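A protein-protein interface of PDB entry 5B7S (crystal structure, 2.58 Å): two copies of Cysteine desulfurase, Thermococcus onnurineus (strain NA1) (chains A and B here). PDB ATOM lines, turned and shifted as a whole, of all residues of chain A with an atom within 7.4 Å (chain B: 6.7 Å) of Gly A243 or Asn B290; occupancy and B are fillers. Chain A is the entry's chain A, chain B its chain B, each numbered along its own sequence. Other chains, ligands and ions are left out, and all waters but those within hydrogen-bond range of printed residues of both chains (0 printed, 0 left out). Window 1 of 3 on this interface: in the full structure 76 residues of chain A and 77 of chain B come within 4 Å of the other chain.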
ATOM      1  N   MET A  56     -29.428 -25.418  29.193  1.00  0.00           N
ATOM      2  CA  MET A  56     -30.142 -25.784  27.963  1.00  0.00           C
ATOM      3  C   MET A  56     -31.322 -26.649  28.291  1.00  0.00           C
ATOM      4  O   MET A  56     -32.400 -26.479  27.755  1.00  0.00           O
ATOM      5  CB  MET A  56     -29.233 -26.507  26.963  1.00  0.00           C
ATOM      6  CG  MET A  56     -28.253 -25.593  26.244  1.00  0.00           C
ATOM      7  SD  MET A  56     -26.856 -26.483  25.568  1.00  0.00           S
ATOM      8  CE  MET A  56     -27.386 -26.683  23.877  1.00  0.00           C
ATOM      9  N   TYR A  60     -35.330 -26.412  27.170  1.00  0.00           N
ATOM     10  CA  TYR A  60     -36.071 -27.483  26.451  1.00  0.00           C
ATOM     11  C   TYR A  60     -37.201 -28.105  27.258  1.00  0.00           C
ATOM     12  O   TYR A  60     -38.230 -28.493  26.698  1.00  0.00           O
ATOM     13  CB  TYR A  60     -35.127 -28.585  25.927  1.00  0.00           C
ATOM     14  CG  TYR A  60     -34.293 -28.138  24.760  1.00  0.00           C
ATOM     15  CD1 TYR A  60     -34.893 -27.834  23.552  1.00  0.00           C
ATOM     16  CD2 TYR A  60     -32.891 -28.011  24.859  1.00  0.00           C
ATOM     17  CE1 TYR A  60     -34.153 -27.410  22.459  1.00  0.00           C
ATOM     18  CE2 TYR A  60     -32.135 -27.587  23.771  1.00  0.00           C
ATOM     19  CZ  TYR A  60     -32.783 -27.285  22.570  1.00  0.00           C
ATOM     20  OH  TYR A  60     -32.085 -26.842  21.475  1.00  0.00           O
ATOM     21  N   PHE A 102     -26.054 -14.121  15.808  1.00  0.00           N
ATOM     22  CA  PHE A 102     -25.765 -15.527  16.061  1.00  0.00           C
ATOM     23  C   PHE A 102     -25.727 -16.327  14.784  1.00  0.00           C
ATOM     24  O   PHE A 102     -26.523 -16.117  13.892  1.00  0.00           O
ATOM     25  CB  PHE A 102     -26.796 -16.129  17.004  1.00  0.00           C
ATOM     26  CG  PHE A 102     -26.697 -15.633  18.422  1.00  0.00           C
ATOM     27  CD1 PHE A 102     -25.575 -15.893  19.187  1.00  0.00           C
ATOM     28  CD2 PHE A 102     -27.742 -14.947  19.006  1.00  0.00           C
ATOM     29  CE1 PHE A 102     -25.485 -15.453  20.489  1.00  0.00           C
ATOM     30  CE2 PHE A 102     -27.665 -14.498  20.314  1.00  0.00           C
ATOM     31  CZ  PHE A 102     -26.529 -14.752  21.054  1.00  0.00           C
ATOM     32  N   THR A 103     -24.824 -17.284  14.728  1.00  0.00           N
ATOM     33  CA  THR A 103     -24.630 -18.148  13.569  1.00  0.00           C
ATOM     34  C   THR A 103     -24.460 -19.583  14.073  1.00  0.00           C
ATOM     35  O   THR A 103     -24.553 -19.811  15.267  1.00  0.00           O
ATOM     36  CB  THR A 103     -23.376 -17.702  12.789  1.00  0.00           C
ATOM     37  OG1 THR A 103     -22.212 -17.825  13.611  1.00  0.00           O
ATOM     38  CG2 THR A 103     -23.498 -16.258  12.328  1.00  0.00           C
ATOM     39  N   LYS A 104     -24.217 -20.553  13.185  1.00  0.00           N
ATOM     40  CA  LYS A 104     -23.995 -21.952  13.591  1.00  0.00           C
ATOM     41  C   LYS A 104     -22.542 -22.181  14.073  1.00  0.00           C
ATOM     42  O   LYS A 104     -22.282 -23.006  14.975  1.00  0.00           O
ATOM     43  CB  LYS A 104     -24.414 -22.930  12.469  1.00  0.00           C
ATOM     44  CG  LYS A 104     -23.285 -23.529  11.600  1.00  0.00           C
ATOM     45  CD  LYS A 104     -23.778 -24.521  10.536  1.00  0.00           C
ATOM     46  CE  LYS A 104     -24.868 -23.982   9.622  1.00  0.00           C
ATOM     47  NZ  LYS A 104     -24.439 -22.741   8.914  1.00  0.00           N
ATOM     48  N   ASN A 105     -21.600 -21.445  13.487  1.00  0.00           N
ATOM     49  CA  ASN A 105     -20.202 -21.516  13.897  1.00  0.00           C
ATOM     50  C   ASN A 105     -19.364 -20.404  13.320  1.00  0.00           C
ATOM     51  O   ASN A 105     -19.850 -19.604  12.522  1.00  0.00           O
ATOM     52  CB  ASN A 105     -19.608 -22.854  13.474  1.00  0.00           C
ATOM     53  CG  ASN A 105     -19.802 -23.157  11.999  1.00  0.00           C
ATOM     54  OD1 ASN A 105     -19.648 -22.300  11.143  1.00  0.00           O
ATOM     55  ND2 ASN A 105     -20.116 -24.408  11.706  1.00  0.00           N
ATOM     56  N   GLU A 108     -19.401 -20.010   9.434  1.00  0.00           N
ATOM     57  CA  GLU A 108     -20.569 -19.255   8.928  1.00  0.00           C
ATOM     58  C   GLU A 108     -20.297 -17.773   9.100  1.00  0.00           C
ATOM     59  O   GLU A 108     -20.415 -17.040   8.144  1.00  0.00           O
ATOM     60  CB  GLU A 108     -21.890 -19.635   9.624  1.00  0.00           C
ATOM     61  CG  GLU A 108     -23.054 -18.732   9.255  1.00  0.00           C
ATOM     62  CD  GLU A 108     -24.423 -19.209   9.733  1.00  0.00           C
ATOM     63  OE1 GLU A 108     -24.563 -20.392  10.102  1.00  0.00           O
ATOM     64  OE2 GLU A 108     -25.381 -18.395   9.739  1.00  0.00           O
ATOM     65  N   GLY A 234     -18.889 -20.926  19.973  1.00  0.00           N
ATOM     66  CA  GLY A 234     -19.223 -21.292  21.346  1.00  0.00           C
ATOM     67  C   GLY A 234     -18.734 -22.637  21.849  1.00  0.00           C
ATOM     68  O   GLY A 234     -18.561 -22.803  23.061  1.00  0.00           O
ATOM     69  N   HIS A 235     -18.512 -23.592  20.935  1.00  0.00           N
ATOM     70  CA  HIS A 235     -18.103 -24.950  21.296  1.00  0.00           C
ATOM     71  C   HIS A 235     -16.611 -25.094  21.644  1.00  0.00           C
ATOM     72  O   HIS A 235     -16.199 -26.088  22.187  1.00  0.00           O
ATOM     73  CB  HIS A 235     -18.527 -25.962  20.224  1.00  0.00           C
ATOM     74  CG  HIS A 235     -17.786 -25.839  18.941  1.00  0.00           C
ATOM     75  ND1 HIS A 235     -16.588 -26.481  18.713  1.00  0.00           N
ATOM     76  CD2 HIS A 235     -18.077 -25.156  17.805  1.00  0.00           C
ATOM     77  CE1 HIS A 235     -16.153 -26.158  17.504  1.00  0.00           C
ATOM     78  NE2 HIS A 235     -17.053 -25.380  16.926  1.00  0.00           N
ATOM     79  N   GLY A 240     -19.241 -23.776  25.527  1.00  0.00           N
ATOM     80  CA  GLY A 240     -20.657 -23.824  25.139  1.00  0.00           C
ATOM     81  C   GLY A 240     -20.996 -25.050  24.301  1.00  0.00           C
ATOM     82  O   GLY A 240     -20.148 -25.909  24.070  1.00  0.00           O
ATOM     83  N   PRO A 241     -22.246 -25.137  23.846  1.00  0.00           N
ATOM     84  CA  PRO A 241     -22.649 -26.227  22.958  1.00  0.00           C
ATOM     85  C   PRO A 241     -22.213 -26.013  21.513  1.00  0.00           C
ATOM     86  O   PRO A 241     -21.765 -24.934  21.141  1.00  0.00           O
ATOM     87  CB  PRO A 241     -24.178 -26.169  23.031  1.00  0.00           C
ATOM     88  CG  PRO A 241     -24.465 -24.707  23.218  1.00  0.00           C
ATOM     89  CD  PRO A 241     -23.322 -24.143  24.033  1.00  0.00           C
ATOM     90  N   THR A 242     -22.427 -27.038  20.709  1.00  0.00           N
ATOM     91  CA  THR A 242     -22.229 -27.002  19.268  1.00  0.00           C
ATOM     92  C   THR A 242     -23.378 -26.255  18.589  1.00  0.00           C
ATOM     93  O   THR A 242     -24.433 -26.012  19.179  1.00  0.00           O
ATOM     94  CB  THR A 242     -22.200 -28.452  18.698  1.00  0.00           C
ATOM     95  OG1 THR A 242     -23.349 -29.184  19.145  1.00  0.00           O
ATOM     96  CG2 THR A 242     -20.968 -29.212  19.184  1.00  0.00           C
ATOM     97  N   GLY A 243     -23.180 -25.882  17.344  1.00  0.00           N
ATOM     98  CA  GLY A 243     -24.207 -25.193  16.605  1.00  0.00           C
ATOM     99  C   GLY A 243     -24.443 -23.756  17.006  1.00  0.00           C
ATOM    100  O   GLY A 243     -25.467 -23.173  16.652  1.00  0.00           O
ATOM    101  N   ILE A 244     -23.516 -23.153  17.720  1.00  0.00           N
ATOM    102  CA  ILE A 244     -23.693 -21.761  18.038  1.00  0.00           C
ATOM    103  C   ILE A 244     -22.387 -20.997  17.796  1.00  0.00           C
ATOM    104  O   ILE A 244     -21.321 -21.386  18.266  1.00  0.00           O
ATOM    105  CB  ILE A 244     -24.296 -21.578  19.454  1.00  0.00           C
ATOM    106  CG1 ILE A 244     -24.769 -20.124  19.675  1.00  0.00           C
ATOM    107  CG2 ILE A 244     -23.304 -21.961  20.534  1.00  0.00           C
ATOM    108  CD1 ILE A 244     -25.788 -19.570  18.686  1.00  0.00           C
ATOM    109  N   GLY A 245     -22.496 -19.936  17.016  1.00  0.00           N
ATOM    110  CA  GLY A 245     -21.395 -19.085  16.645  1.00  0.00           C
ATOM    111  C   GLY A 245     -21.817 -17.645  16.756  1.00  0.00           C
ATOM    112  O   GLY A 245     -23.000 -17.330  16.857  1.00  0.00           O
ATOM    113  N   ASN A 290     -31.091 -20.634  16.939  1.00  0.00           N
ATOM    114  CA  ASN A 290     -30.768 -21.682  17.874  1.00  0.00           C
ATOM    115  C   ASN A 290     -30.867 -21.094  19.300  1.00  0.00           C
ATOM    116  O   ASN A 290     -29.900 -20.708  19.888  1.00  0.00           O
ATOM    117  CB  ASN A 290     -29.383 -22.203  17.582  1.00  0.00           C
ATOM    118  CG  ASN A 290     -28.995 -23.363  18.478  1.00  0.00           C
ATOM    119  OD1 ASN A 290     -29.799 -23.853  19.333  1.00  0.00           O
ATOM    120  ND2 ASN A 290     -27.746 -23.818  18.308  1.00  0.00           N
ATOM    121  N   GLY A 293     -28.873 -23.074  21.962  1.00  0.00           N
ATOM    122  CA  GLY A 293     -27.442 -22.850  21.883  1.00  0.00           C
ATOM    123  C   GLY A 293     -26.993 -21.496  22.391  1.00  0.00           C
ATOM    124  O   GLY A 293     -25.912 -21.368  22.990  1.00  0.00           O
ATOM    125  N   ALA A 294     -27.829 -20.495  22.159  1.00  0.00           N
ATOM    126  CA  ALA A 294     -27.579 -19.167  22.639  1.00  0.00           C
ATOM    127  C   ALA A 294     -27.594 -19.168  24.160  1.00  0.00           C
ATOM    128  O   ALA A 294     -26.683 -18.662  24.811  1.00  0.00           O
ATOM    129  CB  ALA A 294     -28.627 -18.207  22.081  1.00  0.00           C
ATOM    130  N   MET B  56     -29.139 -35.794  23.706  1.00  0.00           N
ATOM    131  CA  MET B  56     -28.208 -34.682  23.545  1.00  0.00           C
ATOM    132  C   MET B  56     -27.268 -34.647  24.729  1.00  0.00           C
ATOM    133  O   MET B  56     -26.089 -34.427  24.577  1.00  0.00           O
ATOM    134  CB  MET B  56     -28.935 -33.331  23.449  1.00  0.00           C
ATOM    135  CG  MET B  56     -29.614 -33.038  22.125  1.00  0.00           C
ATOM    136  SD  MET B  56     -30.594 -31.510  22.116  1.00  0.00           S
ATOM    137  CE  MET B  56     -29.334 -30.262  22.444  1.00  0.00           C
ATOM    138  N   TYR B  60     -23.109 -34.484  25.057  1.00  0.00           N
ATOM    139  CA  TYR B  60     -22.331 -33.407  25.682  1.00  0.00           C
ATOM    140  C   TYR B  60     -21.499 -33.869  26.922  1.00  0.00           C
ATOM    141  O   TYR B  60     -20.451 -33.306  27.186  1.00  0.00           O
ATOM    142  CB  TYR B  60     -23.212 -32.181  26.011  1.00  0.00           C
ATOM    143  CG  TYR B  60     -23.644 -31.322  24.820  1.00  0.00           C
ATOM    144  CD1 TYR B  60     -22.717 -30.596  24.077  1.00  0.00           C
ATOM    145  CD2 TYR B  60     -24.992 -31.157  24.496  1.00  0.00           C
ATOM    146  CE1 TYR B  60     -23.108 -29.805  22.998  1.00  0.00           C
ATOM    147  CE2 TYR B  60     -25.384 -30.348  23.428  1.00  0.00           C
ATOM    148  CZ  TYR B  60     -24.436 -29.680  22.674  1.00  0.00           C
ATOM    149  OH  TYR B  60     -24.843 -28.893  21.606  1.00  0.00           O
ATOM    150  N   TYR B  82     -22.860 -38.842  14.652  1.00  0.00           N
ATOM    151  CA  TYR B  82     -23.194 -37.802  13.703  1.00  0.00           C
ATOM    152  C   TYR B  82     -23.640 -38.363  12.350  1.00  0.00           C
ATOM    153  O   TYR B  82     -24.638 -37.942  11.781  1.00  0.00           O
ATOM    154  CB  TYR B  82     -22.003 -36.863  13.540  1.00  0.00           C
ATOM    155  CG  TYR B  82     -22.299 -35.665  12.655  1.00  0.00           C
ATOM    156  CD1 TYR B  82     -23.323 -34.775  12.966  1.00  0.00           C
ATOM    157  CD2 TYR B  82     -21.515 -35.387  11.525  1.00  0.00           C
ATOM    158  CE1 TYR B  82     -23.588 -33.680  12.149  1.00  0.00           C
ATOM    159  CE2 TYR B  82     -21.782 -34.293  10.717  1.00  0.00           C
ATOM    160  CZ  TYR B  82     -22.828 -33.450  11.033  1.00  0.00           C
ATOM    161  OH  TYR B  82     -23.090 -32.373  10.217  1.00  0.00           O
ATOM    162  N   PHE B 102     -26.961 -30.467   6.850  1.00  0.00           N
ATOM    163  CA  PHE B 102     -27.386 -29.751   8.053  1.00  0.00           C
ATOM    164  C   PHE B 102     -27.108 -28.248   7.971  1.00  0.00           C
ATOM    165  O   PHE B 102     -26.070 -27.814   7.475  1.00  0.00           O
ATOM    166  CB  PHE B 102     -26.791 -30.390   9.302  1.00  0.00           C
ATOM    167  CG  PHE B 102     -27.256 -31.808   9.507  1.00  0.00           C
ATOM    168  CD1 PHE B 102     -28.602 -32.092   9.631  1.00  0.00           C
ATOM    169  CD2 PHE B 102     -26.358 -32.858   9.538  1.00  0.00           C
ATOM    170  CE1 PHE B 102     -29.048 -33.386   9.798  1.00  0.00           C
ATOM    171  CE2 PHE B 102     -26.795 -34.180   9.710  1.00  0.00           C
ATOM    172  CZ  PHE B 102     -28.147 -34.445   9.846  1.00  0.00           C
ATOM    173  N   THR B 103     -28.100 -27.485   8.425  1.00  0.00           N
ATOM    174  CA  THR B 103     -28.110 -26.038   8.478  1.00  0.00           C
ATOM    175  C   THR B 103     -28.702 -25.628   9.839  1.00  0.00           C
ATOM    176  O   THR B 103     -29.088 -26.515  10.629  1.00  0.00           O
ATOM    177  CB  THR B 103     -29.068 -25.503   7.425  1.00  0.00           C
ATOM    178  OG1 THR B 103     -30.407 -25.948   7.745  1.00  0.00           O
ATOM    179  CG2 THR B 103     -28.636 -25.943   5.990  1.00  0.00           C
ATOM    180  N   LYS B 104     -28.832 -24.325  10.119  1.00  0.00           N
ATOM    181  CA  LYS B 104     -29.351 -23.895  11.423  1.00  0.00           C
ATOM    182  C   LYS B 104     -30.879 -23.977  11.458  1.00  0.00           C
ATOM    183  O   LYS B 104     -31.480 -24.362  12.476  1.00  0.00           O
ATOM    184  CB  LYS B 104     -28.790 -22.535  11.854  1.00  0.00           C
ATOM    185  CG  LYS B 104     -29.743 -21.346  11.838  1.00  0.00           C
ATOM    186  CD  LYS B 104     -29.082 -20.129  12.458  1.00  0.00           C
ATOM    187  CE  LYS B 104     -28.379 -19.239  11.460  1.00  0.00           C
ATOM    188  NZ  LYS B 104     -27.524 -19.909  10.450  1.00  0.00           N
ATOM    189  N   PRO B 241     -34.196 -30.461  18.692  1.00  0.00           N
ATOM    190  CA  PRO B 241     -33.783 -29.193  19.283  1.00  0.00           C
ATOM    191  C   PRO B 241     -33.810 -28.062  18.281  1.00  0.00           C
ATOM    192  O   PRO B 241     -34.097 -28.302  17.098  1.00  0.00           O
ATOM    193  CB  PRO B 241     -32.346 -29.474  19.695  1.00  0.00           C
ATOM    194  CG  PRO B 241     -31.885 -30.432  18.664  1.00  0.00           C
ATOM    195  CD  PRO B 241     -33.044 -31.344  18.450  1.00  0.00           C
ATOM    196  N   THR B 242     -33.499 -26.855  18.766  1.00  0.00           N
ATOM    197  CA  THR B 242     -33.289 -25.647  17.926  1.00  0.00           C
ATOM    198  C   THR B 242     -31.914 -25.709  17.305  1.00  0.00           C
ATOM    199  O   THR B 242     -31.103 -26.528  17.678  1.00  0.00           O
ATOM    200  CB  THR B 242     -33.391 -24.328  18.732  1.00  0.00           C
ATOM    201  OG1 THR B 242     -32.374 -24.272  19.744  1.00  0.00           O
ATOM    202  CG2 THR B 242     -34.750 -24.214  19.407  1.00  0.00           C
ATOM    203  N   GLY B 243     -31.668 -24.859  16.338  1.00  0.00           N
ATOM    204  CA  GLY B 243     -30.388 -24.809  15.659  1.00  0.00           C
ATOM    205  C   GLY B 243     -30.075 -25.948  14.713  1.00  0.00           C
ATOM    206  O   GLY B 243     -28.934 -26.125  14.348  1.00  0.00           O
ATOM    207  N   ILE B 244     -31.062 -26.721  14.308  1.00  0.00           N
ATOM    208  CA  ILE B 244     -30.819 -27.774  13.345  1.00  0.00           C
ATOM    209  C   ILE B 244     -31.905 -27.817  12.261  1.00  0.00           C
ATOM    210  O   ILE B 244     -32.986 -28.324  12.453  1.00  0.00           O
ATOM    211  CB  ILE B 244     -30.590 -29.138  14.029  1.00  0.00           C
ATOM    212  CG1 ILE B 244     -30.031 -30.147  13.032  1.00  0.00           C
ATOM    213  CG2 ILE B 244     -31.842 -29.664  14.708  1.00  0.00           C
ATOM    214  CD1 ILE B 244     -28.568 -29.918  12.704  1.00  0.00           C
ATOM    215  N   GLY B 287     -17.398 -25.911   8.483  1.00  0.00           N
ATOM    216  CA  GLY B 287     -17.038 -25.798   9.891  1.00  0.00           C
ATOM    217  C   GLY B 287     -17.649 -26.886  10.747  1.00  0.00           C
ATOM    218  O   GLY B 287     -18.238 -27.851  10.254  1.00  0.00           O
ATOM    219  N   THR B 288     -17.498 -26.722  12.042  1.00  0.00           N
ATOM    220  CA  THR B 288     -17.970 -27.704  12.988  1.00  0.00           C
ATOM    221  C   THR B 288     -19.473 -27.706  12.889  1.00  0.00           C
ATOM    222  O   THR B 288     -20.111 -26.685  13.134  1.00  0.00           O
ATOM    223  CB  THR B 288     -17.521 -27.356  14.433  1.00  0.00           C
ATOM    224  OG1 THR B 288     -16.093 -27.211  14.464  1.00  0.00           O
ATOM    225  CG2 THR B 288     -17.919 -28.438  15.408  1.00  0.00           C
ATOM    226  N   PRO B 289     -20.052 -28.835  12.494  1.00  0.00           N
ATOM    227  CA  PRO B 289     -21.510 -28.816  12.507  1.00  0.00           C
ATOM    228  C   PRO B 289     -22.073 -28.815  13.920  1.00  0.00           C
ATOM    229  O   PRO B 289     -21.341 -28.992  14.897  1.00  0.00           O
ATOM    230  CB  PRO B 289     -21.885 -30.103  11.773  1.00  0.00           C
ATOM    231  CG  PRO B 289     -20.732 -31.010  12.006  1.00  0.00           C
ATOM    232  CD  PRO B 289     -19.511 -30.141  12.068  1.00  0.00           C
ATOM    233  N   ASN B 290     -23.383 -28.580  14.002  1.00  0.00           N
ATOM    234  CA  ASN B 290     -24.157 -28.764  15.222  1.00  0.00           C
ATOM    235  C   ASN B 290     -24.392 -30.259  15.415  1.00  0.00           C
ATOM    236  O   ASN B 290     -25.493 -30.769  15.145  1.00  0.00           O
ATOM    237  CB  ASN B 290     -25.490 -28.018  15.134  1.00  0.00           C
ATOM    238  CG  ASN B 290     -26.234 -27.963  16.470  1.00  0.00           C
ATOM    239  OD1 ASN B 290     -25.766 -28.478  17.502  1.00  0.00           O
ATOM    240  ND2 ASN B 290     -27.412 -27.340  16.450  1.00  0.00           N
ATOM    241  N   ILE B 291     -23.359 -30.924  15.943  1.00  0.00           N
ATOM    242  CA  ILE B 291     -23.360 -32.361  16.139  1.00  0.00           C
ATOM    243  C   ILE B 291     -24.426 -32.687  17.194  1.00  0.00           C
ATOM    244  O   ILE B 291     -25.253 -33.600  17.021  1.00  0.00           O
ATOM    245  CB  ILE B 291     -21.973 -32.865  16.653  1.00  0.00           C
ATOM    246  CG1 ILE B 291     -20.809 -32.398  15.771  1.00  0.00           C
ATOM    247  CG2 ILE B 291     -21.924 -34.399  16.730  1.00  0.00           C
ATOM    248  CD1 ILE B 291     -19.482 -32.309  16.514  1.00  0.00           C
ATOM    249  N   GLY B 292     -24.388 -31.929  18.299  1.00  0.00           N
ATOM    250  CA  GLY B 292     -25.403 -32.011  19.366  1.00  0.00           C
ATOM    251  C   GLY B 292     -26.826 -31.929  18.851  1.00  0.00           C
ATOM    252  O   GLY B 292     -27.685 -32.697  19.281  1.00  0.00           O
ATOM    253  N   GLY B 293     -27.052 -31.022  17.895  1.00  0.00           N
ATOM    254  CA  GLY B 293     -28.395 -30.758  17.325  1.00  0.00           C
ATOM    255  C   GLY B 293     -28.901 -31.902  16.474  1.00  0.00           C
ATOM    256  O   GLY B 293     -30.047 -32.334  16.611  1.00  0.00           O
ATOM    257  N   ALA B 294     -28.011 -32.389  15.618  1.00  0.00           N
ATOM    258  CA  ALA B 294     -28.260 -33.499  14.708  1.00  0.00           C
ATOM    259  C   ALA B 294     -28.551 -34.783  15.456  1.00  0.00           C
ATOM    260  O   ALA B 294     -29.425 -35.558  15.069  1.00  0.00           O
ATOM    261  CB  ALA B 294     -27.045 -33.698  13.807  1.00  0.00           C
ATOM    262  N   ILE B 295     -27.811 -35.019  16.525  1.00  0.00           N
ATOM    263  CA  ILE B 295     -28.095 -36.161  17.384  1.00  0.00           C
ATOM    264  C   ILE B 295     -29.459 -35.993  18.062  1.00  0.00           C
ATOM    265  O   ILE B 295     -30.238 -36.953  18.148  1.00  0.00           O
ATOM    266  CB  ILE B 295     -26.952 -36.372  18.394  1.00  0.00           C
ATOM    267  CG1 ILE B 295     -25.701 -36.847  17.642  1.00  0.00           C
ATOM    268  CG2 ILE B 295     -27.349 -37.384  19.465  1.00  0.00           C
ATOM    269  CD1 ILE B 295     -24.414 -36.767  18.440  1.00  0.00           C
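OD1 of Asn B290 sits at hydrogen-bond distance from N of Gly B293.
O of Gly A243 is in hydrogen-bond range of ND2 of Asn A290 (2.9 Å).
O of Gly B243 is in hydrogen-bond range of ND2 of Asn B290 (2.9 Å).
The side-chain amino group (NZ) of Lys A104 is in salt-bridge range of the side-chain carboxylate (OE1) of Glu A108 (2.6 Å).
The backbone carbonyl oxygen (O) of Asn A105 sits at hydrogen-bond distance from the side-chain hydroxyl (OG1) of Thr A103, at 3.2 Å.
The backbone NH (N) of Gly A293 is in hydrogen-bond range of the side-chain amide oxygen (OD1) of Asn A290, at 2.9 Å.
Of chain B, only Asn B290 (3.4 Å) comes within 4 Å of Gly A243.
Of the printed residues of chain A, Asn B290 touches Thr A242 (3.0 Å), Gly A243 (3.4 Å) and Asn A290 (3.996 Å).
Of the printed residues of chain A, Gly B243 touches Asn A290.
Of the printed residues of chain A, Gly B287 touches Asn A105 (3.6 Å).
Printed residues of chain B within 4 Å of Glu A108: Lys B104 (2.7 Å).
Of the printed residues of chain A, Thr B288 touches Asn A105 and His A235.
Of the printed residues of chain A, Pro B289 touches Thr A242.
Ala B294 touches none of the printed residues of chain A.
Thr B103 touches none of the printed residues of chain A.
The nearest printed residue of chain A that does not touch Asn B290 is Lys A104 (5.4 Å).
The nearest printed residue of chain A that does not touch Gly B292 is Gly A243 (6.2 Å).
The side-chain amide oxygen of Asn A290 sits at hydrogen-bond distance from the side-chain hydroxyl of Thr B242 (2.6 Å).
The side-chain hydroxyl of Thr A242 sits at hydrogen-bond distance from the backbone NH of Gly B292 (3.1 Å).
OG1 of Thr A242 is in hydrogen-bond range of OH of Tyr B60 (2.9 Å).
The side-chain hydroxyl (OH) of Tyr A60 lies within hydrogen-bond range of the backbone NH (N) of Thr B242, at 3.1 Å.
The side-chain amide nitrogen (ND2) of Asn A105 is in hydrogen-bond range of the backbone carbonyl oxygen (O) of Thr B288 (2.7 Å).
The side-chain hydroxyl of Thr A242 sits at hydrogen-bond distance from the side-chain amide oxygen of Asn B290 (3.0 Å).
The side-chain carboxylate (OE2) of Glu A108 lies within salt-bridge range of the side-chain amino group (NZ) of Lys B104.
A ring nitrogen (NE2) of His A235 sits at hydrogen-bond distance from the side-chain hydroxyl (OG1) of Thr B288 (3.2 Å).
CB of Pro B241 touches OH of Tyr A60, at 3.2 Å.
C of Gly B287 touches ND2 of Asn A105 (3.6 Å).
OH of Tyr B60 touches CB of Pro A241 (3.1 Å).
Pro B289 touches Thr A242 (O to CB, 3.9 Å).
N of Ile B291 touches OG1 of Thr A242, at 3.6 Å.
Gly A243 touches Asn B290 (CA to CB, 3.4 Å).
CB of Asn A290 touches CA of Gly B243, 3.4 Å away.
Asn A290 touches Asn B290.
Tyr A60 touches Pro B241, and with the chains exchanged Pro A241 touches Tyr B60.
Tyr A60 touches Thr B242, and with the chains exchanged Thr A242 touches Tyr B60.
Thr A242 touches Asn B290, and with the chains exchanged Asn A290 touches Thr B242.
Asn A290 touches its own counterpart, Asn B290.
Positions printed for both chains: 56, 60, 102, 103, 104, 241, 242, 243, 244, 290, 293 and 294.
Hydrophobic or aromatic side chains of chain B within 4 Å of the printed part of chain A: Tyr B60 and Pro B241.
Hydrophobic or aromatic side chains of chain A that line the printed part of chain B: Tyr A60, His A235 and Pro A241.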
